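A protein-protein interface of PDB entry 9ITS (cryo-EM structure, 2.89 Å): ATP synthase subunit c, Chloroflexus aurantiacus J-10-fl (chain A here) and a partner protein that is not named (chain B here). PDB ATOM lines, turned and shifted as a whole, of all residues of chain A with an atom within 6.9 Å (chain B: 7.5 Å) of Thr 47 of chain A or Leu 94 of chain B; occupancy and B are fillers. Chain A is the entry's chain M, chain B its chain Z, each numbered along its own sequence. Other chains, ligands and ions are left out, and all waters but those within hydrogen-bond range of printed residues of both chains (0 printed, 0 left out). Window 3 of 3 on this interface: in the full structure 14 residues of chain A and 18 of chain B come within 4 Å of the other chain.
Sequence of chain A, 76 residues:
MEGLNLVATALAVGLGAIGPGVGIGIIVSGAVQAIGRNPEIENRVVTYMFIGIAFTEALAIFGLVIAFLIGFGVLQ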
ATOM      1  N   GLU A  42     -17.864 -28.332 -35.040  1.00  0.00           N
ATOM      2  CA  GLU A  42     -18.669 -28.073 -33.847  1.00  0.00           C
ATOM      3  C   GLU A  42     -17.808 -27.707 -32.641  1.00  0.00           C
ATOM      4  O   GLU A  42     -18.173 -26.821 -31.856  1.00  0.00           O
ATOM      5  CB  GLU A  42     -19.534 -29.298 -33.543  1.00  0.00           C
ATOM      6  CG  GLU A  42     -20.006 -29.408 -32.106  1.00  0.00           C
ATOM      7  CD  GLU A  42     -20.839 -30.649 -31.865  1.00  0.00           C
ATOM      8  OE1 GLU A  42     -21.264 -31.281 -32.855  1.00  0.00           O
ATOM      9  OE2 GLU A  42     -21.064 -30.996 -30.688  1.00  0.00           O
ATOM     10  N   ASN A  43     -16.667 -28.381 -32.475  1.00  0.00           N
ATOM     11  CA  ASN A  43     -15.804 -28.108 -31.329  1.00  0.00           C
ATOM     12  C   ASN A  43     -15.269 -26.682 -31.351  1.00  0.00           C
ATOM     13  O   ASN A  43     -15.106 -26.065 -30.293  1.00  0.00           O
ATOM     14  CB  ASN A  43     -14.652 -29.113 -31.288  1.00  0.00           C
ATOM     15  CG  ASN A  43     -13.917 -29.213 -32.611  1.00  0.00           C
ATOM     16  OD1 ASN A  43     -14.352 -28.658 -33.619  1.00  0.00           O
ATOM     17  ND2 ASN A  43     -12.794 -29.922 -32.611  1.00  0.00           N
ATOM     18  N   ARG A  44     -14.985 -26.146 -32.537  1.00  0.00           N
ATOM     19  CA  ARG A  44     -14.565 -24.753 -32.643  1.00  0.00           C
ATOM     20  C   ARG A  44     -15.739 -23.796 -32.452  1.00  0.00           C
ATOM     21  O   ARG A  44     -15.539 -22.645 -32.047  1.00  0.00           O
ATOM     22  CB  ARG A  44     -13.894 -24.525 -34.002  1.00  0.00           C
ATOM     23  CG  ARG A  44     -13.344 -23.128 -34.233  1.00  0.00           C
ATOM     24  CD  ARG A  44     -12.171 -22.843 -33.310  1.00  0.00           C
ATOM     25  NE  ARG A  44     -10.976 -23.570 -33.718  1.00  0.00           N
ATOM     26  CZ  ARG A  44      -9.788 -23.447 -33.143  1.00  0.00           C
ATOM     27  NH1 ARG A  44      -9.596 -22.627 -32.122  1.00  0.00           N
ATOM     28  NH2 ARG A  44      -8.767 -24.164 -33.601  1.00  0.00           N
ATOM     29  N   VAL A  45     -16.962 -24.263 -32.706  1.00  0.00           N
ATOM     30  CA  VAL A  45     -18.136 -23.393 -32.670  1.00  0.00           C
ATOM     31  C   VAL A  45     -18.636 -23.205 -31.241  1.00  0.00           C
ATOM     32  O   VAL A  45     -19.006 -22.091 -30.842  1.00  0.00           O
ATOM     33  CB  VAL A  45     -19.236 -23.962 -33.585  1.00  0.00           C
ATOM     34  CG1 VAL A  45     -20.560 -23.287 -33.318  1.00  0.00           C
ATOM     35  CG2 VAL A  45     -18.854 -23.771 -35.039  1.00  0.00           C
ATOM     36  N   VAL A  46     -18.653 -24.287 -30.457  1.00  0.00           N
ATOM     37  CA  VAL A  46     -19.329 -24.278 -29.157  1.00  0.00           C
ATOM     38  C   VAL A  46     -18.694 -23.262 -28.213  1.00  0.00           C
ATOM     39  O   VAL A  46     -19.388 -22.621 -27.412  1.00  0.00           O
ATOM     40  CB  VAL A  46     -19.336 -25.697 -28.555  1.00  0.00           C
ATOM     41  CG1 VAL A  46     -19.786 -25.675 -27.104  1.00  0.00           C
ATOM     42  CG2 VAL A  46     -20.244 -26.603 -29.368  1.00  0.00           C
ATOM     43  N   THR A  47     -17.372 -23.093 -28.292  1.00  0.00           N
ATOM     44  CA  THR A  47     -16.692 -22.129 -27.431  1.00  0.00           C
ATOM     45  C   THR A  47     -17.191 -20.710 -27.685  1.00  0.00           C
ATOM     46  O   THR A  47     -17.514 -19.970 -26.748  1.00  0.00           O
ATOM     47  CB  THR A  47     -15.181 -22.209 -27.655  1.00  0.00           C
ATOM     48  OG1 THR A  47     -14.857 -21.634 -28.926  1.00  0.00           O
ATOM     49  CG2 THR A  47     -14.726 -23.654 -27.648  1.00  0.00           C
ATOM     50  N   TYR A  48     -17.286 -20.322 -28.957  1.00  0.00           N
ATOM     51  CA  TYR A  48     -17.744 -18.975 -29.278  1.00  0.00           C
ATOM     52  C   TYR A  48     -19.231 -18.823 -28.989  1.00  0.00           C
ATOM     53  O   TYR A  48     -19.697 -17.730 -28.639  1.00  0.00           O
ATOM     54  CB  TYR A  48     -17.429 -18.655 -30.737  1.00  0.00           C
ATOM     55  CG  TYR A  48     -15.957 -18.417 -30.969  1.00  0.00           C
ATOM     56  CD1 TYR A  48     -15.365 -17.211 -30.623  1.00  0.00           C
ATOM     57  CD2 TYR A  48     -15.153 -19.413 -31.507  1.00  0.00           C
ATOM     58  CE1 TYR A  48     -14.017 -16.996 -30.822  1.00  0.00           C
ATOM     59  CE2 TYR A  48     -13.805 -19.207 -31.708  1.00  0.00           C
ATOM     60  CZ  TYR A  48     -13.244 -17.997 -31.364  1.00  0.00           C
ATOM     61  OH  TYR A  48     -11.900 -17.791 -31.562  1.00  0.00           O
ATOM     62  N   MET A  49     -19.992 -19.912 -29.122  1.00  0.00           N
ATOM     63  CA  MET A  49     -21.401 -19.874 -28.740  1.00  0.00           C
ATOM     64  C   MET A  49     -21.550 -19.591 -27.249  1.00  0.00           C
ATOM     65  O   MET A  49     -22.369 -18.758 -26.843  1.00  0.00           O
ATOM     66  CB  MET A  49     -22.091 -21.185 -29.122  1.00  0.00           C
ATOM     67  CG  MET A  49     -23.437 -21.407 -28.441  1.00  0.00           C
ATOM     68  SD  MET A  49     -24.153 -23.034 -28.760  1.00  0.00           S
ATOM     69  CE  MET A  49     -23.217 -24.052 -27.640  1.00  0.00           C
ATOM     70  N   PHE A  50     -20.748 -20.264 -26.418  1.00  0.00           N
ATOM     71  CA  PHE A  50     -20.737 -19.964 -24.987  1.00  0.00           C
ATOM     72  C   PHE A  50     -20.279 -18.541 -24.706  1.00  0.00           C
ATOM     73  O   PHE A  50     -20.786 -17.899 -23.785  1.00  0.00           O
ATOM     74  CB  PHE A  50     -19.859 -20.952 -24.215  1.00  0.00           C
ATOM     75  CG  PHE A  50     -20.404 -22.349 -24.146  1.00  0.00           C
ATOM     76  CD1 PHE A  50     -21.721 -22.618 -24.467  1.00  0.00           C
ATOM     77  CD2 PHE A  50     -19.600 -23.391 -23.716  1.00  0.00           C
ATOM     78  CE1 PHE A  50     -22.219 -23.904 -24.368  1.00  0.00           C
ATOM     79  CE2 PHE A  50     -20.094 -24.678 -23.628  1.00  0.00           C
ATOM     80  CZ  PHE A  50     -21.403 -24.933 -23.960  1.00  0.00           C
ATOM     81  N   ILE A  51     -19.313 -18.035 -25.475  1.00  0.00           N
ATOM     82  CA  ILE A  51     -18.867 -16.652 -25.281  1.00  0.00           C
ATOM     83  C   ILE A  51     -20.021 -15.683 -25.524  1.00  0.00           C
ATOM     84  O   ILE A  51     -20.269 -14.762 -24.730  1.00  0.00           O
ATOM     85  CB  ILE A  51     -17.664 -16.338 -26.187  1.00  0.00           C
ATOM     86  CG1 ILE A  51     -16.430 -17.119 -25.733  1.00  0.00           C
ATOM     87  CG2 ILE A  51     -17.373 -14.846 -26.196  1.00  0.00           C
ATOM     88  CD1 ILE A  51     -15.324 -17.155 -26.759  1.00  0.00           C
ATOM     89  N   GLY A  52     -20.755 -15.888 -26.617  1.00  0.00           N
ATOM     90  CA  GLY A  52     -21.889 -15.023 -26.904  1.00  0.00           C
ATOM     91  C   GLY A  52     -22.998 -15.138 -25.874  1.00  0.00           C
ATOM     92  O   GLY A  52     -23.582 -14.130 -25.458  1.00  0.00           O
ATOM     93  N   LEU B  88      -9.759 -32.689 -16.203  1.00  0.00           N
ATOM     94  CA  LEU B  88      -8.515 -31.990 -16.507  1.00  0.00           C
ATOM     95  C   LEU B  88      -8.114 -32.187 -17.963  1.00  0.00           C
ATOM     96  O   LEU B  88      -7.666 -31.241 -18.620  1.00  0.00           O
ATOM     97  CB  LEU B  88      -7.404 -32.462 -15.571  1.00  0.00           C
ATOM     98  CG  LEU B  88      -7.443 -31.876 -14.159  1.00  0.00           C
ATOM     99  CD1 LEU B  88      -6.641 -32.738 -13.200  1.00  0.00           C
ATOM    100  CD2 LEU B  88      -6.932 -30.446 -14.154  1.00  0.00           C
ATOM    101  N   GLU B  89      -8.275 -33.406 -18.484  1.00  0.00           N
ATOM    102  CA  GLU B  89      -7.997 -33.656 -19.895  1.00  0.00           C
ATOM    103  C   GLU B  89      -8.933 -32.858 -20.791  1.00  0.00           C
ATOM    104  O   GLU B  89      -8.505 -32.301 -21.810  1.00  0.00           O
ATOM    105  CB  GLU B  89      -8.118 -35.150 -20.196  1.00  0.00           C
ATOM    106  CG  GLU B  89      -7.797 -35.525 -21.634  1.00  0.00           C
ATOM    107  CD  GLU B  89      -6.321 -35.770 -21.860  1.00  0.00           C
ATOM    108  OE1 GLU B  89      -5.651 -36.260 -20.928  1.00  0.00           O
ATOM    109  OE2 GLU B  89      -5.828 -35.473 -22.969  1.00  0.00           O
ATOM    110  N   SER B  90     -10.218 -32.793 -20.427  1.00  0.00           N
ATOM    111  CA  SER B  90     -11.174 -32.025 -21.217  1.00  0.00           C
ATOM    112  C   SER B  90     -10.816 -30.545 -21.234  1.00  0.00           C
ATOM    113  O   SER B  90     -10.839 -29.906 -22.293  1.00  0.00           O
ATOM    114  CB  SER B  90     -12.587 -32.230 -20.670  1.00  0.00           C
ATOM    115  OG  SER B  90     -12.885 -33.609 -20.536  1.00  0.00           O
ATOM    116  N   LEU B  91     -10.465 -29.986 -20.073  1.00  0.00           N
ATOM    117  CA  LEU B  91     -10.075 -28.581 -20.012  1.00  0.00           C
ATOM    118  C   LEU B  91      -8.792 -28.325 -20.792  1.00  0.00           C
ATOM    119  O   LEU B  91      -8.672 -27.305 -21.484  1.00  0.00           O
ATOM    120  CB  LEU B  91      -9.914 -28.144 -18.557  1.00  0.00           C
ATOM    121  CG  LEU B  91     -11.191 -28.023 -17.725  1.00  0.00           C
ATOM    122  CD1 LEU B  91     -10.906 -27.299 -16.422  1.00  0.00           C
ATOM    123  CD2 LEU B  91     -12.284 -27.311 -18.506  1.00  0.00           C
ATOM    124  N   TYR B  92      -7.819 -29.234 -20.687  1.00  0.00           N
ATOM    125  CA  TYR B  92      -6.566 -29.074 -21.415  1.00  0.00           C
ATOM    126  C   TYR B  92      -6.797 -29.104 -22.920  1.00  0.00           C
ATOM    127  O   TYR B  92      -6.230 -28.287 -23.655  1.00  0.00           O
ATOM    128  CB  TYR B  92      -5.582 -30.166 -20.994  1.00  0.00           C
ATOM    129  CG  TYR B  92      -4.216 -30.058 -21.631  1.00  0.00           C
ATOM    130  CD1 TYR B  92      -3.300 -29.110 -21.197  1.00  0.00           C
ATOM    131  CD2 TYR B  92      -3.838 -30.911 -22.660  1.00  0.00           C
ATOM    132  CE1 TYR B  92      -2.047 -29.009 -21.774  1.00  0.00           C
ATOM    133  CE2 TYR B  92      -2.589 -30.819 -23.243  1.00  0.00           C
ATOM    134  CZ  TYR B  92      -1.698 -29.866 -22.795  1.00  0.00           C
ATOM    135  OH  TYR B  92      -0.453 -29.771 -23.373  1.00  0.00           O
ATOM    136  N   ASN B  93      -7.641 -30.023 -23.395  1.00  0.00           N
ATOM    137  CA  ASN B  93      -7.967 -30.069 -24.818  1.00  0.00           C
ATOM    138  C   ASN B  93      -8.722 -28.819 -25.253  1.00  0.00           C
ATOM    139  O   ASN B  93      -8.493 -28.301 -26.353  1.00  0.00           O
ATOM    140  CB  ASN B  93      -8.777 -31.325 -25.131  1.00  0.00           C
ATOM    141  CG  ASN B  93      -7.908 -32.558 -25.266  1.00  0.00           C
ATOM    142  OD1 ASN B  93      -6.707 -32.460 -25.519  1.00  0.00           O
ATOM    143  ND2 ASN B  93      -8.511 -33.729 -25.097  1.00  0.00           N
ATOM    144  N   LEU B  94      -9.623 -28.320 -24.403  1.00  0.00           N
ATOM    145  CA  LEU B  94     -10.356 -27.099 -24.723  1.00  0.00           C
ATOM    146  C   LEU B  94      -9.408 -25.919 -24.897  1.00  0.00           C
ATOM    147  O   LEU B  94      -9.469 -25.197 -25.901  1.00  0.00           O
ATOM    148  CB  LEU B  94     -11.378 -26.811 -23.623  1.00  0.00           C
ATOM    149  CG  LEU B  94     -12.323 -25.632 -23.847  1.00  0.00           C
ATOM    150  CD1 LEU B  94     -12.953 -25.722 -25.222  1.00  0.00           C
ATOM    151  CD2 LEU B  94     -13.390 -25.595 -22.766  1.00  0.00           C
ATOM    152  N   PHE B  95      -8.505 -25.721 -23.936  1.00  0.00           N
ATOM    153  CA  PHE B  95      -7.570 -24.606 -24.022  1.00  0.00           C
ATOM    154  C   PHE B  95      -6.537 -24.806 -25.122  1.00  0.00           C
ATOM    155  O   PHE B  95      -6.018 -23.817 -25.650  1.00  0.00           O
ATOM    156  CB  PHE B  95      -6.883 -24.385 -22.674  1.00  0.00           C
ATOM    157  CG  PHE B  95      -7.841 -24.212 -21.530  1.00  0.00           C
ATOM    158  CD1 PHE B  95      -9.032 -23.525 -21.706  1.00  0.00           C
ATOM    159  CD2 PHE B  95      -7.552 -24.730 -20.279  1.00  0.00           C
ATOM    160  CE1 PHE B  95      -9.918 -23.366 -20.661  1.00  0.00           C
ATOM    161  CE2 PHE B  95      -8.436 -24.576 -19.230  1.00  0.00           C
ATOM    162  CZ  PHE B  95      -9.620 -23.893 -19.422  1.00  0.00           C
ATOM    163  N   ARG B  96      -6.229 -26.056 -25.479  1.00  0.00           N
ATOM    164  CA  ARG B  96      -5.405 -26.309 -26.656  1.00  0.00           C
ATOM    165  C   ARG B  96      -6.135 -25.901 -27.928  1.00  0.00           C
ATOM    166  O   ARG B  96      -5.518 -25.399 -28.873  1.00  0.00           O
ATOM    167  CB  ARG B  96      -5.012 -27.785 -26.711  1.00  0.00           C
ATOM    168  CG  ARG B  96      -3.729 -28.060 -27.473  1.00  0.00           C
ATOM    169  CD  ARG B  96      -3.062 -29.330 -26.977  1.00  0.00           C
ATOM    170  NE  ARG B  96      -3.936 -30.490 -27.113  1.00  0.00           N
ATOM    171  CZ  ARG B  96      -3.545 -31.746 -26.944  1.00  0.00           C
ATOM    172  NH1 ARG B  96      -2.293 -32.046 -26.636  1.00  0.00           N
ATOM    173  NH2 ARG B  96      -4.433 -32.726 -27.089  1.00  0.00           N
ATOM    174  N   ASN B  97      -7.449 -26.132 -27.974  1.00  0.00           N
ATOM    175  CA  ASN B  97      -8.242 -25.668 -29.108  1.00  0.00           C
ATOM    176  C   ASN B  97      -8.272 -24.146 -29.175  1.00  0.00           C
ATOM    177  O   ASN B  97      -8.210 -23.568 -30.267  1.00  0.00           O
ATOM    178  CB  ASN B  97      -9.660 -26.232 -29.022  1.00  0.00           C
ATOM    179  CG  ASN B  97      -9.799 -27.567 -29.725  1.00  0.00           C
ATOM    180  OD1 ASN B  97      -9.228 -27.782 -30.794  1.00  0.00           O
ATOM    181  ND2 ASN B  97     -10.562 -28.474 -29.126  1.00  0.00           N
ATOM    182  N   ILE B  98      -8.372 -23.481 -28.023  1.00  0.00           N
ATOM    183  CA  ILE B  98      -8.433 -22.020 -28.020  1.00  0.00           C
ATOM    184  C   ILE B  98      -7.075 -21.421 -28.372  1.00  0.00           C
ATOM    185  O   ILE B  98      -6.967 -20.571 -29.263  1.00  0.00           O
ATOM    186  CB  ILE B  98      -8.939 -21.500 -26.663  1.00  0.00           C
ATOM    187  CG1 ILE B  98     -10.309 -22.090 -26.338  1.00  0.00           C
ATOM    188  CG2 ILE B  98      -9.013 -19.981 -26.677  1.00  0.00           C
ATOM    189  CD1 ILE B  98     -10.523 -22.326 -24.862  1.00  0.00           C
ATOM    190  N   ASN B  99      -6.021 -21.853 -27.683  1.00  0.00           N
ATOM    191  CA  ASN B  99      -4.685 -21.311 -27.882  1.00  0.00           C
ATOM    192  C   ASN B  99      -3.678 -22.447 -27.986  1.00  0.00           C
ATOM    193  O   ASN B  99      -3.899 -23.550 -27.484  1.00  0.00           O
ATOM    194  CB  ASN B  99      -4.288 -20.357 -26.748  1.00  0.00           C
ATOM    195  CG  ASN B  99      -3.304 -19.295 -27.200  1.00  0.00           C
ATOM    196  OD1 ASN B  99      -2.355 -19.582 -27.928  1.00  0.00           O
ATOM    197  ND2 ASN B  99      -3.530 -18.058 -26.773  1.00  0.00           N
ATOM    198  N   VAL B 103      -1.325 -22.652 -23.238  1.00  0.00           N
ATOM    199  CA  VAL B 103      -2.111 -23.543 -22.392  1.00  0.00           C
ATOM    200  C   VAL B 103      -1.401 -23.796 -21.070  1.00  0.00           C
ATOM    201  O   VAL B 103      -2.017 -23.743 -20.001  1.00  0.00           O
ATOM    202  CB  VAL B 103      -2.406 -24.858 -23.134  1.00  0.00           C
ATOM    203  CG1 VAL B 103      -3.396 -25.700 -22.345  1.00  0.00           C
ATOM    204  CG2 VAL B 103      -2.930 -24.570 -24.528  1.00  0.00           C
ATOM    205  N   LEU B 289     -17.858 -23.262 -16.187  1.00  0.00           N
ATOM    206  CA  LEU B 289     -17.251 -23.424 -17.503  1.00  0.00           C
ATOM    207  C   LEU B 289     -17.243 -22.108 -18.271  1.00  0.00           C
ATOM    208  O   LEU B 289     -16.285 -21.813 -18.992  1.00  0.00           O
ATOM    209  CB  LEU B 289     -17.990 -24.504 -18.290  1.00  0.00           C
ATOM    210  CG  LEU B 289     -17.366 -24.932 -19.619  1.00  0.00           C
ATOM    211  CD1 LEU B 289     -16.013 -25.587 -19.389  1.00  0.00           C
ATOM    212  CD2 LEU B 289     -18.298 -25.868 -20.373  1.00  0.00           C
ATOM    213  N   ILE B 290     -18.304 -21.309 -18.124  1.00  0.00           N
ATOM    214  CA  ILE B 290     -18.365 -19.998 -18.765  1.00  0.00           C
ATOM    215  C   ILE B 290     -17.243 -19.104 -18.264  1.00  0.00           C
ATOM    216  O   ILE B 290     -16.543 -18.464 -19.053  1.00  0.00           O
ATOM    217  CB  ILE B 290     -19.742 -19.345 -18.536  1.00  0.00           C
ATOM    218  CG1 ILE B 290     -20.834 -20.062 -19.333  1.00  0.00           C
ATOM    219  CG2 ILE B 290     -19.695 -17.868 -18.858  1.00  0.00           C
ATOM    220  CD1 ILE B 290     -20.619 -20.024 -20.819  1.00  0.00           C
ATOM    221  N   ALA B 292     -14.359 -19.928 -16.866  1.00  0.00           N
ATOM    222  CA  ALA B 292     -13.061 -20.424 -17.317  1.00  0.00           C
ATOM    223  C   ALA B 292     -12.836 -20.133 -18.800  1.00  0.00           C
ATOM    224  O   ALA B 292     -11.789 -19.595 -19.194  1.00  0.00           O
ATOM    225  CB  ALA B 292     -12.955 -21.924 -17.042  1.00  0.00           C
ATOM    226  N   LEU B 293     -13.821 -20.471 -19.637  1.00  0.00           N
ATOM    227  CA  LEU B 293     -13.682 -20.287 -21.075  1.00  0.00           C
ATOM    228  C   LEU B 293     -13.558 -18.814 -21.439  1.00  0.00           C
ATOM    229  O   LEU B 293     -12.749 -18.452 -22.297  1.00  0.00           O
ATOM    230  CB  LEU B 293     -14.872 -20.924 -21.793  1.00  0.00           C
ATOM    231  CG  LEU B 293     -15.060 -20.638 -23.282  1.00  0.00           C
ATOM    232  CD1 LEU B 293     -13.836 -21.045 -24.080  1.00  0.00           C
ATOM    233  CD2 LEU B 293     -16.286 -21.363 -23.795  1.00  0.00           C
ATOM    234  N   LEU B 294     -14.342 -17.949 -20.792  1.00  0.00           N
ATOM    235  CA  LEU B 294     -14.285 -16.526 -21.102  1.00  0.00           C
ATOM    236  C   LEU B 294     -12.970 -15.899 -20.661  1.00  0.00           C
ATOM    237  O   LEU B 294     -12.405 -15.086 -21.397  1.00  0.00           O
ATOM    238  CB  LEU B 294     -15.480 -15.794 -20.488  1.00  0.00           C
ATOM    239  CG  LEU B 294     -16.768 -15.742 -21.322  1.00  0.00           C
ATOM    240  CD1 LEU B 294     -16.502 -14.931 -22.576  1.00  0.00           C
ATOM    241  CD2 LEU B 294     -17.302 -17.110 -21.719  1.00  0.00           C
ATOM    242  N   TYR B 296     -10.073 -17.457 -20.408  1.00  0.00           N
ATOM    243  CA  TYR B 296      -9.040 -17.949 -21.314  1.00  0.00           C
ATOM    244  C   TYR B 296      -9.156 -17.307 -22.694  1.00  0.00           C
ATOM    245  O   TYR B 296      -8.140 -16.968 -23.314  1.00  0.00           O
ATOM    246  CB  TYR B 296      -9.104 -19.470 -21.421  1.00  0.00           C
ATOM    247  CG  TYR B 296      -7.856 -20.070 -22.022  1.00  0.00           C
ATOM    248  CD1 TYR B 296      -6.710 -20.247 -21.259  1.00  0.00           C
ATOM    249  CD2 TYR B 296      -7.817 -20.441 -23.357  1.00  0.00           C
ATOM    250  CE1 TYR B 296      -5.564 -20.789 -21.810  1.00  0.00           C
ATOM    251  CE2 TYR B 296      -6.679 -20.982 -23.916  1.00  0.00           C
ATOM    252  CZ  TYR B 296      -5.555 -21.154 -23.139  1.00  0.00           C
ATOM    253  OH  TYR B 296      -4.422 -21.693 -23.699  1.00  0.00           O
ATOM    254  N   ALA B 297     -10.383 -17.120 -23.187  1.00  0.00           N
ATOM    255  CA  ALA B 297     -10.574 -16.499 -24.492  1.00  0.00           C
ATOM    256  C   ALA B 297     -10.191 -15.026 -24.465  1.00  0.00           C
ATOM    257  O   ALA B 297      -9.672 -14.497 -25.454  1.00  0.00           O
ATOM    258  CB  ALA B 297     -12.024 -16.668 -24.947  1.00  0.00           C
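The guanidinium group of Arg 44 of chain A lies within hydrogen-bond range of the backbone carbonyl oxygen of Asn 97 of chain B (2.5 Å).
The backbone carbonyl oxygen of Arg 44 of chain A sits at hydrogen-bond distance from the side-chain hydroxyl of Thr 47 of chain A, at 3.4 Å.
The backbone carbonyl oxygen (O) of Asn 93 of chain B is in hydrogen-bond range of the side-chain amide nitrogen (ND2) of Asn 97 of chain B.
Of the 20 printed residues of chain B, 7 touch a printed residue of chain A.
Printed residues of chain A that touch a printed residue of chain B: Arg 44, Thr 47, Phe 50 and Ile 51.
Along chain A the printed residues that touch a printed residue of chain B span positions 44 to 51.
Among the printed residues, no Asp or Glu carboxylate lies within 4 Å of a Lys or Arg side-chain nitrogen of the other chain.
Among the printed residues, pairs that only touch across the chains: Thr 47 of chain A with Leu 293 of chain B (3.5 Å), Phe 50 of chain A with Ile 290 of chain B (3.6 Å), Phe 50 of chain A with Leu 293 of chain B (3.6 Å), Thr 47 of chain A with Leu 94 of chain B (3.6 Å), Ile 51 of chain A with Leu 294 of chain B (3.7 Å), Ile 51 of chain A with Ala 297 of chain B (3.8 Å) and Phe 50 of chain A with Leu 289 of chain B (3.9 Å).
Thr 47 of chain A touches just these residues of chain B: Leu 94 and Leu 293.
Printed residues of chain B within 4 Å of Ile 51 of chain A: Leu 294 and Ala 297.
Of the printed residues of chain A, Leu 289 of chain B touches Phe 50 (3.9 Å).
Glu 42 of chain A touches none of the printed residues of chain B.
Met 49 of chain A touches none of the printed residues of chain B.
The nearest residue of chain B that does not touch Thr 47 of chain A is Ile 98 of chain B (4.9 Å).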
